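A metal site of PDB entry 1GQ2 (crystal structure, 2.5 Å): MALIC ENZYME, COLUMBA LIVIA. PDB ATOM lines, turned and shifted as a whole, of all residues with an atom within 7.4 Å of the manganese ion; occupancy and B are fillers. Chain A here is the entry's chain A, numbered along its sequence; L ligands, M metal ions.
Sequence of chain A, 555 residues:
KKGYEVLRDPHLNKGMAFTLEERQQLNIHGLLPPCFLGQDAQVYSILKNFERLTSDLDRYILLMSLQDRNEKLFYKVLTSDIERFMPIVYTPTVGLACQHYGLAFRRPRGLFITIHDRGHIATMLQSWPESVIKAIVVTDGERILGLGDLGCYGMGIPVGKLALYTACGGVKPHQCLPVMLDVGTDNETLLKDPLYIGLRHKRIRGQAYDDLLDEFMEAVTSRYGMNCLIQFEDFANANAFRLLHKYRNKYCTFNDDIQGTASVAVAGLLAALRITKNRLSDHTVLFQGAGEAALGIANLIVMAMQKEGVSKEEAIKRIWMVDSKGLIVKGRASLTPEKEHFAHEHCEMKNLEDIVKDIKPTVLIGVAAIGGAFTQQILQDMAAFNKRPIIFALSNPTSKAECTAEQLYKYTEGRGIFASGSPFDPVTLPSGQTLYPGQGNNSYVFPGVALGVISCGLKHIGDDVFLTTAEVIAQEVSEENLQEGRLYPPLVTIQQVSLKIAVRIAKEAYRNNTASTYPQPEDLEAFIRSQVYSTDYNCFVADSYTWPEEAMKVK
O8 of LG2 L2 is in salt-bridge range of NH2 of Arg 143. N of Glu 292 lies within hydrogen-bond range of O9 of LG2 L2. O13 of LG2 L2 sits at hydrogen-bond distance from N of Asn 396 (2.8 Å). An oxygen (O13) of LG2 L2 sits at hydrogen-bond distance from the backbone carbonyl oxygen (O) of Asn 396 (3.2 Å). The side-chain amide nitrogen (ND2) of Asn 396 lies within hydrogen-bond range of an oxygen (O14) of LG2 L2 (3.3 Å).
The backbone NH (N) of Asp 257 lies within hydrogen-bond range of the side-chain amide oxygen (OD1) of Asn 255. NZ of Lys 161 lies within salt-bridge range of OE1 of Glu 233. OE1 of Glu 233 sits close to OD2 of Asp 256, at 2.6 Å. NE2 of Gln 231 is in hydrogen-bond range of OE1 of Glu 233. The backbone carbonyl oxygen (O) of Asp 234 sits at hydrogen-bond distance from the backbone NH (N) of Arg 143, at 3.4 Å. The side-chain amino group (NZ) of Lys 161 sits close to the side-chain amide nitrogen (ND2) of Asn 442 (3.4 Å). The side-chain amino group (NZ) of Lys 161 lies within salt-bridge range of the side-chain carboxylate (OD2) of Asp 256 (2.6 Å). The side-chain hydroxyl (OH) of Tyr 90 lies within hydrogen-bond range of the side-chain amino group (NZ) of Lys 161, at 3.3 Å.
Lys 161 touches the manganese ion (NZ to MN, 3.6 Å). Four residues have an atom within 4 Å of the manganese ion: Lys 161, Glu 233, Asp 234 and Asp 257. The nearest printed residue that does not touch the manganese ion is Arg 143 (4.2 Å).
The manganese ion is bound by the side-chain carboxylate (OD1) of Asp 257 (2.3 Å), an oxygen (O2) of LIG L1 (2.3 Å), the side-chain carboxylate (OE2) of Glu 233 (2.4 Å), the side-chain carboxylate (OD1) of Asp 234 (2.4 Å) and an oxygen (O3) of LIG L1 (2.5 Å).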
ATOM      1  N   TYR A  90     -13.691  11.584   4.530  1.00  0.00           N
ATOM      2  CA  TYR A  90     -12.742  12.161   3.571  1.00  0.00           C
ATOM      3  C   TYR A  90     -11.302  11.936   4.067  1.00  0.00           C
ATOM      4  O   TYR A  90     -11.058  10.977   4.800  1.00  0.00           O
ATOM      5  CB  TYR A  90     -13.035  13.658   3.436  1.00  0.00           C
ATOM      6  CG  TYR A  90     -12.537  14.351   2.187  1.00  0.00           C
ATOM      7  CD1 TYR A  90     -12.932  13.923   0.917  1.00  0.00           C
ATOM      8  CD2 TYR A  90     -11.733  15.480   2.277  1.00  0.00           C
ATOM      9  CE1 TYR A  90     -12.530  14.613  -0.222  1.00  0.00           C
ATOM     10  CE2 TYR A  90     -11.336  16.174   1.145  1.00  0.00           C
ATOM     11  CZ  TYR A  90     -11.739  15.737  -0.097  1.00  0.00           C
ATOM     12  OH  TYR A  90     -11.327  16.417  -1.222  1.00  0.00           O
ATOM     13  N   ARG A 143      -3.737   7.453  -9.496  1.00  0.00           N
ATOM     14  CA  ARG A 143      -3.062   8.413  -8.618  1.00  0.00           C
ATOM     15  C   ARG A 143      -4.007   8.801  -7.463  1.00  0.00           C
ATOM     16  O   ARG A 143      -4.522   9.920  -7.424  1.00  0.00           O
ATOM     17  CB  ARG A 143      -2.650   9.649  -9.426  1.00  0.00           C
ATOM     18  CG  ARG A 143      -1.548  10.485  -8.803  1.00  0.00           C
ATOM     19  CD  ARG A 143      -2.030  11.219  -7.577  1.00  0.00           C
ATOM     20  NE  ARG A 143      -2.702  12.467  -7.918  1.00  0.00           N
ATOM     21  CZ  ARG A 143      -3.565  13.090  -7.112  1.00  0.00           C
ATOM     22  NH1 ARG A 143      -3.854  12.577  -5.926  1.00  0.00           N
ATOM     23  NH2 ARG A 143      -4.109  14.237  -7.476  1.00  0.00           N
ATOM     24  N   ILE A 144      -4.223   7.866  -6.551  1.00  0.00           N
ATOM     25  CA  ILE A 144      -5.097   8.069  -5.396  1.00  0.00           C
ATOM     26  C   ILE A 144      -4.337   8.801  -4.300  1.00  0.00           C
ATOM     27  O   ILE A 144      -3.508   8.210  -3.626  1.00  0.00           O
ATOM     28  CB  ILE A 144      -5.598   6.716  -4.851  1.00  0.00           C
ATOM     29  CG1 ILE A 144      -6.294   5.929  -5.977  1.00  0.00           C
ATOM     30  CG2 ILE A 144      -6.563   6.933  -3.677  1.00  0.00           C
ATOM     31  CD1 ILE A 144      -7.595   6.552  -6.443  1.00  0.00           C
ATOM     32  N   LEU A 145      -4.663  10.077  -4.113  1.00  0.00           N
ATOM     33  CA  LEU A 145      -3.969  10.875  -3.107  1.00  0.00           C
ATOM     34  C   LEU A 145      -2.475  10.724  -3.371  1.00  0.00           C
ATOM     35  O   LEU A 145      -2.045  10.609  -4.526  1.00  0.00           O
ATOM     36  CB  LEU A 145      -4.301  10.385  -1.702  1.00  0.00           C
ATOM     37  CG  LEU A 145      -5.775  10.438  -1.251  1.00  0.00           C
ATOM     38  CD1 LEU A 145      -5.902   9.859   0.156  1.00  0.00           C
ATOM     39  CD2 LEU A 145      -6.264  11.875  -1.273  1.00  0.00           C
ATOM     40  N   ILE A 157     -12.523   6.996  -3.312  1.00  0.00           N
ATOM     41  CA  ILE A 157     -12.363   8.428  -3.509  1.00  0.00           C
ATOM     42  C   ILE A 157     -13.599   9.136  -4.089  1.00  0.00           C
ATOM     43  O   ILE A 157     -14.086  10.097  -3.511  1.00  0.00           O
ATOM     44  CB  ILE A 157     -11.128   8.729  -4.403  1.00  0.00           C
ATOM     45  CG1 ILE A 157      -9.854   8.274  -3.682  1.00  0.00           C
ATOM     46  CG2 ILE A 157     -11.063  10.216  -4.733  1.00  0.00           C
ATOM     47  CD1 ILE A 157      -9.669   8.826  -2.269  1.00  0.00           C
ATOM     48  N   LYS A 161     -15.594  12.240  -2.324  1.00  0.00           N
ATOM     49  CA  LYS A 161     -15.885  13.515  -2.951  1.00  0.00           C
ATOM     50  C   LYS A 161     -17.390  13.775  -2.929  1.00  0.00           C
ATOM     51  O   LYS A 161     -17.861  14.765  -2.385  1.00  0.00           O
ATOM     52  CB  LYS A 161     -15.372  13.508  -4.389  1.00  0.00           C
ATOM     53  CG  LYS A 161     -13.871  13.352  -4.490  1.00  0.00           C
ATOM     54  CD  LYS A 161     -13.132  14.590  -3.986  1.00  0.00           C
ATOM     55  CE  LYS A 161     -11.634  14.332  -3.943  1.00  0.00           C
ATOM     56  NZ  LYS A 161     -10.862  15.529  -4.396  1.00  0.00           N
ATOM     57  N   GLN A 231     -16.570  15.303 -13.223  1.00  0.00           N
ATOM     58  CA  GLN A 231     -15.396  15.688 -12.465  1.00  0.00           C
ATOM     59  C   GLN A 231     -14.326  14.603 -12.424  1.00  0.00           C
ATOM     60  O   GLN A 231     -14.497  13.565 -11.777  1.00  0.00           O
ATOM     61  CB  GLN A 231     -15.788  16.030 -11.028  1.00  0.00           C
ATOM     62  CG  GLN A 231     -14.644  16.573 -10.221  1.00  0.00           C
ATOM     63  CD  GLN A 231     -14.963  16.593  -8.756  1.00  0.00           C
ATOM     64  OE1 GLN A 231     -15.961  17.189  -8.329  1.00  0.00           O
ATOM     65  NE2 GLN A 231     -14.119  15.953  -7.970  1.00  0.00           N
ATOM     66  N   PHE A 232     -13.218  14.856 -13.118  1.00  0.00           N
ATOM     67  CA  PHE A 232     -12.107  13.913 -13.133  1.00  0.00           C
ATOM     68  C   PHE A 232     -11.376  13.995 -11.799  1.00  0.00           C
ATOM     69  O   PHE A 232     -11.078  15.091 -11.307  1.00  0.00           O
ATOM     70  CB  PHE A 232     -11.133  14.224 -14.260  1.00  0.00           C
ATOM     71  CG  PHE A 232     -11.656  13.876 -15.622  1.00  0.00           C
ATOM     72  CD1 PHE A 232     -12.576  14.695 -16.267  1.00  0.00           C
ATOM     73  CD2 PHE A 232     -11.233  12.707 -16.247  1.00  0.00           C
ATOM     74  CE1 PHE A 232     -13.064  14.363 -17.528  1.00  0.00           C
ATOM     75  CE2 PHE A 232     -11.706  12.360 -17.502  1.00  0.00           C
ATOM     76  CZ  PHE A 232     -12.619  13.186 -18.146  1.00  0.00           C
ATOM     77  N   GLU A 233     -11.075  12.848 -11.215  1.00  0.00           N
ATOM     78  CA  GLU A 233     -10.390  12.827  -9.937  1.00  0.00           C
ATOM     79  C   GLU A 233      -9.352  11.717  -9.891  1.00  0.00           C
ATOM     80  O   GLU A 233      -9.594  10.607 -10.347  1.00  0.00           O
ATOM     81  CB  GLU A 233     -11.404  12.619  -8.806  1.00  0.00           C
ATOM     82  CG  GLU A 233     -10.853  12.817  -7.401  1.00  0.00           C
ATOM     83  CD  GLU A 233     -10.884  14.268  -6.971  1.00  0.00           C
ATOM     84  OE1 GLU A 233     -11.994  14.840  -6.868  1.00  0.00           O
ATOM     85  OE2 GLU A 233      -9.803  14.855  -6.730  1.00  0.00           O
ATOM     86  N   ASP A 234      -8.195  12.065  -9.347  1.00  0.00           N
ATOM     87  CA  ASP A 234      -7.080  11.145  -9.177  1.00  0.00           C
ATOM     88  C   ASP A 234      -6.678  10.236 -10.343  1.00  0.00           C
ATOM     89  O   ASP A 234      -6.661   9.014 -10.209  1.00  0.00           O
ATOM     90  CB  ASP A 234      -7.324  10.332  -7.912  1.00  0.00           C
ATOM     91  CG  ASP A 234      -7.296  11.200  -6.687  1.00  0.00           C
ATOM     92  OD1 ASP A 234      -6.656  12.275  -6.789  1.00  0.00           O
ATOM     93  OD2 ASP A 234      -7.878  10.839  -5.637  1.00  0.00           O
ATOM     94  N   PHE A 235      -6.378  10.856 -11.473  1.00  0.00           N
ATOM     95  CA  PHE A 235      -5.897  10.174 -12.675  1.00  0.00           C
ATOM     96  C   PHE A 235      -4.406  10.491 -12.669  1.00  0.00           C
ATOM     97  O   PHE A 235      -3.968  11.434 -11.989  1.00  0.00           O
ATOM     98  CB  PHE A 235      -6.504  10.758 -13.960  1.00  0.00           C
ATOM     99  CG  PHE A 235      -7.791  10.115 -14.394  1.00  0.00           C
ATOM    100  CD1 PHE A 235      -8.924  10.172 -13.586  1.00  0.00           C
ATOM    101  CD2 PHE A 235      -7.876   9.459 -15.624  1.00  0.00           C
ATOM    102  CE1 PHE A 235     -10.118   9.579 -14.008  1.00  0.00           C
ATOM    103  CE2 PHE A 235      -9.065   8.861 -16.039  1.00  0.00           C
ATOM    104  CZ  PHE A 235     -10.191   8.925 -15.231  1.00  0.00           C
ATOM    105  N   ASN A 255     -11.012  19.099 -13.953  1.00  0.00           N
ATOM    106  CA  ASN A 255     -10.192  18.146 -13.190  1.00  0.00           C
ATOM    107  C   ASN A 255      -9.939  18.679 -11.784  1.00  0.00           C
ATOM    108  O   ASN A 255      -9.197  19.641 -11.598  1.00  0.00           O
ATOM    109  CB  ASN A 255      -8.852  17.937 -13.900  1.00  0.00           C
ATOM    110  CG  ASN A 255      -8.016  16.845 -13.278  1.00  0.00           C
ATOM    111  OD1 ASN A 255      -7.682  16.890 -12.084  1.00  0.00           O
ATOM    112  ND2 ASN A 255      -7.668  15.850 -14.081  1.00  0.00           N
ATOM    113  N   ASP A 256     -10.542  18.031 -10.783  1.00  0.00           N
ATOM    114  CA  ASP A 256     -10.396  18.488  -9.412  1.00  0.00           C
ATOM    115  C   ASP A 256      -8.957  18.653  -8.905  1.00  0.00           C
ATOM    116  O   ASP A 256      -8.657  19.611  -8.199  1.00  0.00           O
ATOM    117  CB  ASP A 256     -11.179  17.536  -8.487  1.00  0.00           C
ATOM    118  CG  ASP A 256     -11.283  18.051  -7.063  1.00  0.00           C
ATOM    119  OD1 ASP A 256     -11.014  19.248  -6.850  1.00  0.00           O
ATOM    120  OD2 ASP A 256     -11.633  17.264  -6.161  1.00  0.00           O
ATOM    121  N   ASP A 257      -8.075  17.726  -9.272  1.00  0.00           N
ATOM    122  CA  ASP A 257      -6.676  17.743  -8.830  1.00  0.00           C
ATOM    123  C   ASP A 257      -5.830  18.856  -9.412  1.00  0.00           C
ATOM    124  O   ASP A 257      -4.857  19.283  -8.792  1.00  0.00           O
ATOM    125  CB  ASP A 257      -6.011  16.403  -9.166  1.00  0.00           C
ATOM    126  CG  ASP A 257      -6.846  15.212  -8.750  1.00  0.00           C
ATOM    127  OD1 ASP A 257      -6.911  14.927  -7.533  1.00  0.00           O
ATOM    128  OD2 ASP A 257      -7.437  14.568  -9.646  1.00  0.00           O
ATOM    129  N   GLU A 292       0.341  17.638 -11.498  1.00  0.00           N
ATOM    130  CA  GLU A 292      -1.010  18.147 -11.638  1.00  0.00           C
ATOM    131  C   GLU A 292      -1.296  19.348 -10.731  1.00  0.00           C
ATOM    132  O   GLU A 292      -1.691  20.409 -11.194  1.00  0.00           O
ATOM    133  CB  GLU A 292      -2.023  17.043 -11.328  1.00  0.00           C
ATOM    134  CG  GLU A 292      -2.149  15.969 -12.403  1.00  0.00           C
ATOM    135  CD  GLU A 292      -2.934  14.767 -11.915  1.00  0.00           C
ATOM    136  OE1 GLU A 292      -4.023  14.961 -11.312  1.00  0.00           O
ATOM    137  OE2 GLU A 292      -2.481  13.623 -12.142  1.00  0.00           O
ATOM    138  N   ASN A 396      -1.537  14.775   0.431  1.00  0.00           N
ATOM    139  CA  ASN A 396      -2.476  13.936   1.180  1.00  0.00           C
ATOM    140  C   ASN A 396      -2.175  12.454   0.990  1.00  0.00           C
ATOM    141  O   ASN A 396      -1.643  12.038  -0.042  1.00  0.00           O
ATOM    142  CB  ASN A 396      -3.919  14.200   0.743  1.00  0.00           C
ATOM    143  CG  ASN A 396      -4.438  15.518   1.245  1.00  0.00           C
ATOM    144  OD1 ASN A 396      -4.292  15.841   2.418  1.00  0.00           O
ATOM    145  ND2 ASN A 396      -5.073  16.287   0.358  1.00  0.00           N
ATOM    146  N   ASN A 441      -7.704  22.380   0.882  1.00  0.00           N
ATOM    147  CA  ASN A 441      -8.109  21.167   0.169  1.00  0.00           C
ATOM    148  C   ASN A 441      -9.237  21.484  -0.817  1.00  0.00           C
ATOM    149  O   ASN A 441     -10.022  22.415  -0.589  1.00  0.00           O
ATOM    150  CB  ASN A 441      -8.562  20.114   1.182  1.00  0.00           C
ATOM    151  CG  ASN A 441      -8.756  18.745   0.559  1.00  0.00           C
ATOM    152  OD1 ASN A 441      -9.649  18.557  -0.274  1.00  0.00           O
ATOM    153  ND2 ASN A 441      -7.922  17.792   0.968  1.00  0.00           N
ATOM    154  N   ASN A 442      -9.303  20.720  -1.911  1.00  0.00           N
ATOM    155  CA  ASN A 442     -10.342  20.892  -2.936  1.00  0.00           C
ATOM    156  C   ASN A 442     -11.716  21.033  -2.337  1.00  0.00           C
ATOM    157  O   ASN A 442     -12.571  21.732  -2.872  1.00  0.00           O
ATOM    158  CB  ASN A 442     -10.418  19.679  -3.832  1.00  0.00           C
ATOM    159  CG  ASN A 442      -9.144  19.407  -4.540  1.00  0.00           C
ATOM    160  OD1 ASN A 442      -8.577  20.304  -5.175  1.00  0.00           O
ATOM    161  ND2 ASN A 442      -8.674  18.171  -4.444  1.00  0.00           N
HETATM  162  C1  LIG L   1      -5.983  14.715  -3.460  1.00  0.00           C
HETATM  163  C2  LIG L   1      -7.207  15.614  -3.309  1.00  0.00           C
HETATM  164  O1  LIG L   1      -5.320  14.399  -2.480  1.00  0.00           O
HETATM  165  O2  LIG L   1      -7.897  15.933  -4.367  1.00  0.00           O
HETATM  166  O3  LIG L   1      -5.670  14.299  -4.576  1.00  0.00           O
HETATM  167  O4  LIG L   1      -7.558  16.060  -2.128  1.00  0.00           O
HETATM  168  P1  LG2 L   2       1.681  13.945  -9.832  1.00  0.00           P
HETATM  169  O1  LG2 L   2       2.171  12.551  -9.666  1.00  0.00           O
HETATM  170  O2  LG2 L   2       1.088  14.355 -11.125  1.00  0.00           O
HETATM  171  O3  LG2 L   2       2.876  14.976  -9.524  1.00  0.00           O
HETATM  172  C1  LG2 L   2       3.855  14.736  -8.489  1.00  0.00           C
HETATM  173  C2  LG2 L   2       5.027  15.666  -8.738  1.00  0.00           C
HETATM  174  O4  LG2 L   2       5.984  15.601  -7.618  1.00  0.00           O
HETATM  175  C3  LG2 L   2       5.769  15.265  -9.984  1.00  0.00           C
HETATM  176  O5  LG2 L   2       6.055  16.414 -10.806  1.00  0.00           O
HETATM  177  C4  LG2 L   2       7.050  14.673  -9.510  1.00  0.00           C
HETATM  178  O6  LG2 L   2       8.099  14.812 -10.502  1.00  0.00           O
HETATM  179  C5  LG2 L   2       7.312  15.408  -8.221  1.00  0.00           C
HETATM  180  N1  LG2 L   2       8.233  14.703  -7.295  1.00  0.00           N
HETATM  181  C6  LG2 L   2       8.174  13.381  -6.892  1.00  0.00           C
HETATM  182  N2  LG2 L   2       9.175  13.158  -6.005  1.00  0.00           N
HETATM  183  C7  LG2 L   2       9.780  14.317  -5.905  1.00  0.00           C
HETATM  184  C8  LG2 L   2      10.871  14.502  -5.073  1.00  0.00           C
HETATM  185  N3  LG2 L   2      11.384  13.505  -4.349  1.00  0.00           N
HETATM  186  N4  LG2 L   2      11.418  15.758  -5.034  1.00  0.00           N
HETATM  187  C9  LG2 L   2      10.884  16.764  -5.807  1.00  0.00           C
HETATM  188  N5  LG2 L   2       9.809  16.523  -6.620  1.00  0.00           N
HETATM  189  C10 LG2 L   2       9.251  15.277  -6.659  1.00  0.00           C
HETATM  190  O7  LG2 L   2       0.641  14.269  -8.655  1.00  0.00           O
HETATM  191  P2  LG2 L   2      -0.307  15.482  -8.262  1.00  0.00           P
HETATM  192  O8  LG2 L   2      -1.606  15.285  -8.951  1.00  0.00           O
HETATM  193  O9  LG2 L   2       0.423  16.766  -8.464  1.00  0.00           O
HETATM  194  O10 LG2 L   2      -0.513  15.257  -6.685  1.00  0.00           O
HETATM  195  C11 LG2 L   2       0.639  15.171  -5.836  1.00  0.00           C
HETATM  196  C12 LG2 L   2       0.257  15.408  -4.369  1.00  0.00           C
HETATM  197  O11 LG2 L   2      -0.575  16.618  -4.249  1.00  0.00           O
HETATM  198  C13 LG2 L   2      -0.542  14.242  -3.816  1.00  0.00           C
HETATM  199  O12 LG2 L   2       0.095  13.692  -2.628  1.00  0.00           O
HETATM  200  C14 LG2 L   2      -1.920  14.808  -3.466  1.00  0.00           C
HETATM  201  O13 LG2 L   2      -2.424  14.256  -2.224  1.00  0.00           O
HETATM  202  C15 LG2 L   2      -1.706  16.305  -3.381  1.00  0.00           C
HETATM  203  N6  LG2 L   2      -2.934  17.071  -3.739  1.00  0.00           N
HETATM  204  C16 LG2 L   2      -3.578  17.818  -2.729  1.00  0.00           C
HETATM  205  C17 LG2 L   2      -4.757  18.520  -2.997  1.00  0.00           C
HETATM  206  C18 LG2 L   2      -5.429  19.351  -1.864  1.00  0.00           C
HETATM  207  O14 LG2 L   2      -4.917  19.404  -0.750  1.00  0.00           O
HETATM  208  N7  LG2 L   2      -6.543  19.999  -2.203  1.00  0.00           N
HETATM  209  C19 LG2 L   2      -5.308  18.490  -4.309  1.00  0.00           C
HETATM  210  C20 LG2 L   2      -4.674  17.754  -5.347  1.00  0.00           C
HETATM  211  C21 LG2 L   2      -3.489  17.047  -5.072  1.00  0.00           C
HETATM  212  P3  LG2 L   2       8.351  14.250 -12.009  1.00  0.00           P
HETATM  213  O15 LG2 L   2       9.803  14.433 -12.272  1.00  0.00           O
HETATM  214  O16 LG2 L   2       7.932  12.819 -11.954  1.00  0.00           O
HETATM  215  O17 LG2 L   2       7.496  15.081 -12.892  1.00  0.00           O
HETATM  216 MN    MN M   1      -7.869  13.995  -5.649  1.00  0.00          MN
